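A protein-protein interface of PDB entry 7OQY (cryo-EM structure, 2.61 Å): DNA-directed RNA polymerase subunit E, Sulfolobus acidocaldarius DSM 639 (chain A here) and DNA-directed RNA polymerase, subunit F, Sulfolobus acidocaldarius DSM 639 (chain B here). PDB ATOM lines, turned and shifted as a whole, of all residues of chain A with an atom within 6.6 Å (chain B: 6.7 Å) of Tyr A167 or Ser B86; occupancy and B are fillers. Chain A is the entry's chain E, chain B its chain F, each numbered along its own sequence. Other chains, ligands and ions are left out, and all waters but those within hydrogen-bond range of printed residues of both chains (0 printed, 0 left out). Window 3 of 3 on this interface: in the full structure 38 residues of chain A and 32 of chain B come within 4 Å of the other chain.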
ATOM      1  N   VAL A  84     -21.496  -7.380   7.383  1.00  0.00           N
ATOM      2  CA  VAL A  84     -22.626  -7.108   8.262  1.00  0.00           C
ATOM      3  C   VAL A  84     -23.562  -6.149   7.540  1.00  0.00           C
ATOM      4  O   VAL A  84     -23.185  -5.011   7.237  1.00  0.00           O
ATOM      5  CB  VAL A  84     -22.164  -6.525   9.607  1.00  0.00           C
ATOM      6  CG1 VAL A  84     -23.342  -5.942  10.370  1.00  0.00           C
ATOM      7  CG2 VAL A  84     -21.462  -7.588  10.436  1.00  0.00           C
ATOM      8  N   ARG A 143     -30.197  -7.126  11.590  1.00  0.00           N
ATOM      9  CA  ARG A 143     -28.845  -6.825  11.119  1.00  0.00           C
ATOM     10  C   ARG A 143     -28.125  -8.158  10.933  1.00  0.00           C
ATOM     11  O   ARG A 143     -27.542  -8.689  11.882  1.00  0.00           O
ATOM     12  CB  ARG A 143     -28.115  -5.923  12.110  1.00  0.00           C
ATOM     13  CG  ARG A 143     -26.676  -5.609  11.752  1.00  0.00           C
ATOM     14  CD  ARG A 143     -26.065  -4.679  12.785  1.00  0.00           C
ATOM     15  NE  ARG A 143     -26.803  -3.427  12.897  1.00  0.00           N
ATOM     16  CZ  ARG A 143     -26.440  -2.407  13.662  1.00  0.00           C
ATOM     17  NH1 ARG A 143     -25.344  -2.455  14.402  1.00  0.00           N
ATOM     18  NH2 ARG A 143     -27.196  -1.314  13.689  1.00  0.00           N
ATOM     19  N   MET A 145     -25.827 -11.424   9.026  1.00  0.00           N
ATOM     20  CA  MET A 145     -24.433 -11.762   8.777  1.00  0.00           C
ATOM     21  C   MET A 145     -24.354 -12.701   7.582  1.00  0.00           C
ATOM     22  O   MET A 145     -25.144 -13.646   7.478  1.00  0.00           O
ATOM     23  CB  MET A 145     -23.803 -12.418  10.010  1.00  0.00           C
ATOM     24  CG  MET A 145     -22.308 -12.668   9.906  1.00  0.00           C
ATOM     25  SD  MET A 145     -21.353 -11.143   9.823  1.00  0.00           S
ATOM     26  CE  MET A 145     -19.865 -11.722   9.015  1.00  0.00           C
ATOM     27  N   LYS A 164     -25.754 -16.442  15.056  1.00  0.00           N
ATOM     28  CA  LYS A 164     -25.184 -16.935  16.307  1.00  0.00           C
ATOM     29  C   LYS A 164     -24.219 -15.929  16.921  1.00  0.00           C
ATOM     30  O   LYS A 164     -24.076 -15.868  18.148  1.00  0.00           O
ATOM     31  CB  LYS A 164     -24.483 -18.273  16.071  1.00  0.00           C
ATOM     32  CG  LYS A 164     -25.376 -19.344  15.467  1.00  0.00           C
ATOM     33  CD  LYS A 164     -26.408 -19.829  16.471  1.00  0.00           C
ATOM     34  CE  LYS A 164     -25.849 -20.942  17.341  1.00  0.00           C
ATOM     35  NZ  LYS A 164     -26.871 -21.983  17.636  1.00  0.00           N
ATOM     36  N   GLN A 165     -23.549 -15.141  16.090  1.00  0.00           N
ATOM     37  CA  GLN A 165     -22.550 -14.184  16.550  1.00  0.00           C
ATOM     38  C   GLN A 165     -23.191 -13.147  17.468  1.00  0.00           C
ATOM     39  O   GLN A 165     -24.148 -12.475  17.053  1.00  0.00           O
ATOM     40  CB  GLN A 165     -21.912 -13.507  15.336  1.00  0.00           C
ATOM     41  CG  GLN A 165     -20.750 -12.552  15.604  1.00  0.00           C
ATOM     42  CD  GLN A 165     -19.809 -13.024  16.695  1.00  0.00           C
ATOM     43  OE1 GLN A 165     -19.816 -12.499  17.806  1.00  0.00           O
ATOM     44  NE2 GLN A 165     -18.988 -14.019  16.379  1.00  0.00           N
ATOM     45  N   PRO A 166     -22.720 -12.993  18.706  1.00  0.00           N
ATOM     46  CA  PRO A 166     -23.223 -11.912  19.562  1.00  0.00           C
ATOM     47  C   PRO A 166     -22.970 -10.545  18.943  1.00  0.00           C
ATOM     48  O   PRO A 166     -22.223 -10.390  17.974  1.00  0.00           O
ATOM     49  CB  PRO A 166     -22.445 -12.092  20.874  1.00  0.00           C
ATOM     50  CG  PRO A 166     -21.372 -13.111  20.577  1.00  0.00           C
ATOM     51  CD  PRO A 166     -21.910 -13.954  19.470  1.00  0.00           C
ATOM     52  N   TYR A 167     -23.620  -9.538  19.530  1.00  0.00           N
ATOM     53  CA  TYR A 167     -23.681  -8.165  19.032  1.00  0.00           C
ATOM     54  C   TYR A 167     -24.411  -8.064  17.699  1.00  0.00           C
ATOM     55  O   TYR A 167     -24.322  -7.027  17.028  1.00  0.00           O
ATOM     56  CB  TYR A 167     -22.291  -7.527  18.902  1.00  0.00           C
ATOM     57  CG  TYR A 167     -21.469  -7.570  20.170  1.00  0.00           C
ATOM     58  CD1 TYR A 167     -21.922  -6.964  21.334  1.00  0.00           C
ATOM     59  CD2 TYR A 167     -20.236  -8.208  20.201  1.00  0.00           C
ATOM     60  CE1 TYR A 167     -21.174  -6.997  22.495  1.00  0.00           C
ATOM     61  CE2 TYR A 167     -19.481  -8.247  21.357  1.00  0.00           C
ATOM     62  CZ  TYR A 167     -19.954  -7.640  22.502  1.00  0.00           C
ATOM     63  OH  TYR A 167     -19.206  -7.675  23.655  1.00  0.00           O
ATOM     64  N   LEU A 168     -25.128  -9.108  17.294  1.00  0.00           N
ATOM     65  CA  LEU A 168     -25.919  -9.112  16.073  1.00  0.00           C
ATOM     66  C   LEU A 168     -27.326  -9.601  16.381  1.00  0.00           C
ATOM     67  O   LEU A 168     -27.524 -10.435  17.272  1.00  0.00           O
ATOM     68  CB  LEU A 168     -25.283  -9.997  14.992  1.00  0.00           C
ATOM     69  CG  LEU A 168     -24.146  -9.400  14.158  1.00  0.00           C
ATOM     70  CD1 LEU A 168     -22.829  -9.401  14.921  1.00  0.00           C
ATOM     71  CD2 LEU A 168     -24.007 -10.145  12.841  1.00  0.00           C
ATOM     72  N   GLY A 169     -28.299  -9.079  15.645  1.00  0.00           N
ATOM     73  CA  GLY A 169     -29.685  -9.448  15.860  1.00  0.00           C
ATOM     74  C   GLY A 169     -30.593  -8.266  15.573  1.00  0.00           C
ATOM     75  O   GLY A 169     -30.296  -7.430  14.721  1.00  0.00           O
ATOM     76  N   ILE A 174     -29.710  -6.012  20.235  1.00  0.00           N
ATOM     77  CA  ILE A 174     -28.322  -5.582  20.371  1.00  0.00           C
ATOM     78  C   ILE A 174     -28.206  -4.416  21.344  1.00  0.00           C
ATOM     79  O   ILE A 174     -27.204  -4.297  22.061  1.00  0.00           O
ATOM     80  CB  ILE A 174     -27.724  -5.239  18.992  1.00  0.00           C
ATOM     81  CG1 ILE A 174     -28.488  -4.089  18.334  1.00  0.00           C
ATOM     82  CG2 ILE A 174     -27.727  -6.465  18.092  1.00  0.00           C
ATOM     83  CD1 ILE A 174     -27.827  -3.557  17.084  1.00  0.00           C
ATOM     84  N   GLU A 177     -28.227  -5.808  24.766  1.00  0.00           N
ATOM     85  CA  GLU A 177     -26.999  -6.571  24.966  1.00  0.00           C
ATOM     86  C   GLU A 177     -25.825  -5.654  25.284  1.00  0.00           C
ATOM     87  O   GLU A 177     -25.009  -5.958  26.161  1.00  0.00           O
ATOM     88  CB  GLU A 177     -26.702  -7.415  23.726  1.00  0.00           C
ATOM     89  CG  GLU A 177     -25.459  -8.287  23.839  1.00  0.00           C
ATOM     90  CD  GLU A 177     -25.616  -9.410  24.845  1.00  0.00           C
ATOM     91  OE1 GLU A 177     -26.763  -9.844  25.083  1.00  0.00           O
ATOM     92  OE2 GLU A 177     -24.590  -9.860  25.397  1.00  0.00           O
ATOM     93  N   ILE A 178     -25.720  -4.526  24.576  1.00  0.00           N
ATOM     94  CA  ILE A 178     -24.642  -3.577  24.837  1.00  0.00           C
ATOM     95  C   ILE A 178     -24.795  -2.964  26.223  1.00  0.00           C
ATOM     96  O   ILE A 178     -23.817  -2.823  26.968  1.00  0.00           O
ATOM     97  CB  ILE A 178     -24.608  -2.497  23.738  1.00  0.00           C
ATOM     98  CG1 ILE A 178     -24.107  -3.091  22.421  1.00  0.00           C
ATOM     99  CG2 ILE A 178     -23.728  -1.328  24.158  1.00  0.00           C
ATOM    100  CD1 ILE A 178     -22.726  -3.695  22.512  1.00  0.00           C
ATOM    101  N   ALA A 181     -23.870  -5.467  28.847  1.00  0.00           N
ATOM    102  CA  ALA A 181     -22.492  -5.945  28.768  1.00  0.00           C
ATOM    103  C   ALA A 181     -21.590  -5.201  29.746  1.00  0.00           C
ATOM    104  O   ALA A 181     -20.730  -5.811  30.391  1.00  0.00           O
ATOM    105  CB  ALA A 181     -21.968  -5.805  27.339  1.00  0.00           C
ATOM    106  N   GLU B  82     -17.975  -1.667  20.853  1.00  0.00           N
ATOM    107  CA  GLU B  82     -18.088  -3.087  21.161  1.00  0.00           C
ATOM    108  C   GLU B  82     -18.513  -3.935  19.967  1.00  0.00           C
ATOM    109  O   GLU B  82     -18.372  -5.160  20.024  1.00  0.00           O
ATOM    110  CB  GLU B  82     -19.078  -3.294  22.312  1.00  0.00           C
ATOM    111  CG  GLU B  82     -18.916  -2.321  23.478  1.00  0.00           C
ATOM    112  CD  GLU B  82     -17.643  -2.537  24.286  1.00  0.00           C
ATOM    113  OE1 GLU B  82     -16.831  -3.416  23.930  1.00  0.00           O
ATOM    114  OE2 GLU B  82     -17.456  -1.816  25.288  1.00  0.00           O
ATOM    115  N   GLU B  83     -19.027  -3.327  18.896  1.00  0.00           N
ATOM    116  CA  GLU B  83     -19.461  -4.079  17.727  1.00  0.00           C
ATOM    117  C   GLU B  83     -18.654  -3.792  16.470  1.00  0.00           C
ATOM    118  O   GLU B  83     -18.923  -4.411  15.434  1.00  0.00           O
ATOM    119  CB  GLU B  83     -20.948  -3.816  17.436  1.00  0.00           C
ATOM    120  CG  GLU B  83     -21.225  -2.512  16.711  1.00  0.00           C
ATOM    121  CD  GLU B  83     -22.678  -2.090  16.808  1.00  0.00           C
ATOM    122  OE1 GLU B  83     -23.162  -1.877  17.939  1.00  0.00           O
ATOM    123  OE2 GLU B  83     -23.336  -1.971  15.753  1.00  0.00           O
ATOM    124  N   VAL B  84     -17.684  -2.877  16.523  1.00  0.00           N
ATOM    125  CA  VAL B  84     -16.826  -2.634  15.366  1.00  0.00           C
ATOM    126  C   VAL B  84     -16.021  -3.881  15.029  1.00  0.00           C
ATOM    127  O   VAL B  84     -15.868  -4.244  13.857  1.00  0.00           O
ATOM    128  CB  VAL B  84     -15.916  -1.418  15.622  1.00  0.00           C
ATOM    129  CG1 VAL B  84     -14.839  -1.322  14.552  1.00  0.00           C
ATOM    130  CG2 VAL B  84     -16.741  -0.146  15.652  1.00  0.00           C
ATOM    131  N   ARG B  85     -15.496  -4.559  16.054  1.00  0.00           N
ATOM    132  CA  ARG B  85     -14.736  -5.782  15.820  1.00  0.00           C
ATOM    133  C   ARG B  85     -15.597  -6.860  15.172  1.00  0.00           C
ATOM    134  O   ARG B  85     -15.076  -7.723  14.455  1.00  0.00           O
ATOM    135  CB  ARG B  85     -14.147  -6.290  17.137  1.00  0.00           C
ATOM    136  CG  ARG B  85     -13.664  -5.184  18.061  1.00  0.00           C
ATOM    137  CD  ARG B  85     -12.446  -5.617  18.861  1.00  0.00           C
ATOM    138  NE  ARG B  85     -11.226  -5.583  18.063  1.00  0.00           N
ATOM    139  CZ  ARG B  85     -10.560  -4.477  17.761  1.00  0.00           C
ATOM    140  NH1 ARG B  85     -10.964  -3.289  18.182  1.00  0.00           N
ATOM    141  NH2 ARG B  85      -9.460  -4.564  17.018  1.00  0.00           N
ATOM    142  N   SER B  86     -16.910  -6.830  15.412  1.00  0.00           N
ATOM    143  CA  SER B  86     -17.806  -7.753  14.725  1.00  0.00           C
ATOM    144  C   SER B  86     -17.914  -7.412  13.244  1.00  0.00           C
ATOM    145  O   SER B  86     -18.017  -8.311  12.400  1.00  0.00           O
ATOM    146  CB  SER B  86     -19.186  -7.733  15.385  1.00  0.00           C
ATOM    147  OG  SER B  86     -19.118  -8.196  16.722  1.00  0.00           O
ATOM    148  N   VAL B  87     -17.898  -6.120  12.912  1.00  0.00           N
ATOM    149  CA  VAL B  87     -17.907  -5.711  11.510  1.00  0.00           C
ATOM    150  C   VAL B  87     -16.600  -6.101  10.833  1.00  0.00           C
ATOM    151  O   VAL B  87     -16.584  -6.490   9.659  1.00  0.00           O
ATOM    152  CB  VAL B  87     -18.175  -4.198  11.398  1.00  0.00           C
ATOM    153  CG1 VAL B  87     -18.350  -3.793   9.943  1.00  0.00           C
ATOM    154  CG2 VAL B  87     -19.398  -3.813  12.214  1.00  0.00           C
ATOM    155  N   LEU B  88     -15.486  -6.005  11.558  1.00  0.00           N
ATOM    156  CA  LEU B  88     -14.186  -6.327  10.986  1.00  0.00           C
ATOM    157  C   LEU B  88     -14.087  -7.814  10.674  1.00  0.00           C
ATOM    158  O   LEU B  88     -14.374  -8.663  11.524  1.00  0.00           O
ATOM    159  CB  LEU B  88     -13.072  -5.915  11.949  1.00  0.00           C
ATOM    160  CG  LEU B  88     -12.925  -4.423  12.251  1.00  0.00           C
ATOM    161  CD1 LEU B  88     -11.557  -4.134  12.849  1.00  0.00           C
ATOM    162  CD2 LEU B  88     -13.150  -3.592  10.997  1.00  0.00           C
ATOM    163  N   VAL B  89     -13.678  -8.125   9.446  1.00  0.00           N
ATOM    164  CA  VAL B  89     -13.468  -9.504   9.016  1.00  0.00           C
ATOM    165  C   VAL B  89     -12.078  -9.615   8.407  1.00  0.00           C
ATOM    166  O   VAL B  89     -11.803 -10.526   7.617  1.00  0.00           O
ATOM    167  CB  VAL B  89     -14.551  -9.955   8.019  1.00  0.00           C
ATOM    168  CG1 VAL B  89     -15.919  -9.960   8.685  1.00  0.00           C
ATOM    169  CG2 VAL B  89     -14.551  -9.052   6.794  1.00  0.00           C
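NH1 of Arg A143 lies within salt-bridge range of OE2 of Glu B83.
The backbone NH (N) of Arg A143 is in hydrogen-bond range of the backbone carbonyl oxygen (O) of Gly A169, 3.1 Å away.
Among the printed residues, pairs that only touch across the chains: Tyr A167 with Glu B82 (3.5 Å), Tyr A167 with Ser B86 (3.7 Å) and Ile A178 with Glu B82 (3.7 Å).
Of chain B, only Glu B82 (3.5 Å) and Ser B86 (3.7 Å) come within 4 Å of Tyr A167. Printed residues of chain A within 4 Å of Ser B86: Tyr A167. Of the printed residues of chain B, Arg A143 touches Glu B83 (2.5 Å). Of the printed residues of chain A, Glu B83 touches Arg A143 (2.5 Å). The nearest residue of chain B that does not touch Tyr A167 is Glu B83 (4.2 Å). The nearest printed residue of chain A that does not touch Ser B86 is Pro A166 (4.003 Å). The nearest printed residue of chain A that does not touch Glu B82 is Ala A181 (6.0 Å).
Printed residues of chain B that touch a printed residue of chain A: Glu B82, Glu B83 and Ser B86. Printed residues of chain A that touch a printed residue of chain B: Arg A143, Tyr A167 and Ile A178. Hydrophobic or aromatic side chains of chain A within 4 Å of the printed part of chain B: Tyr A167 and Ile A178. Among the printed residues, 4 pairs touch across the chains.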
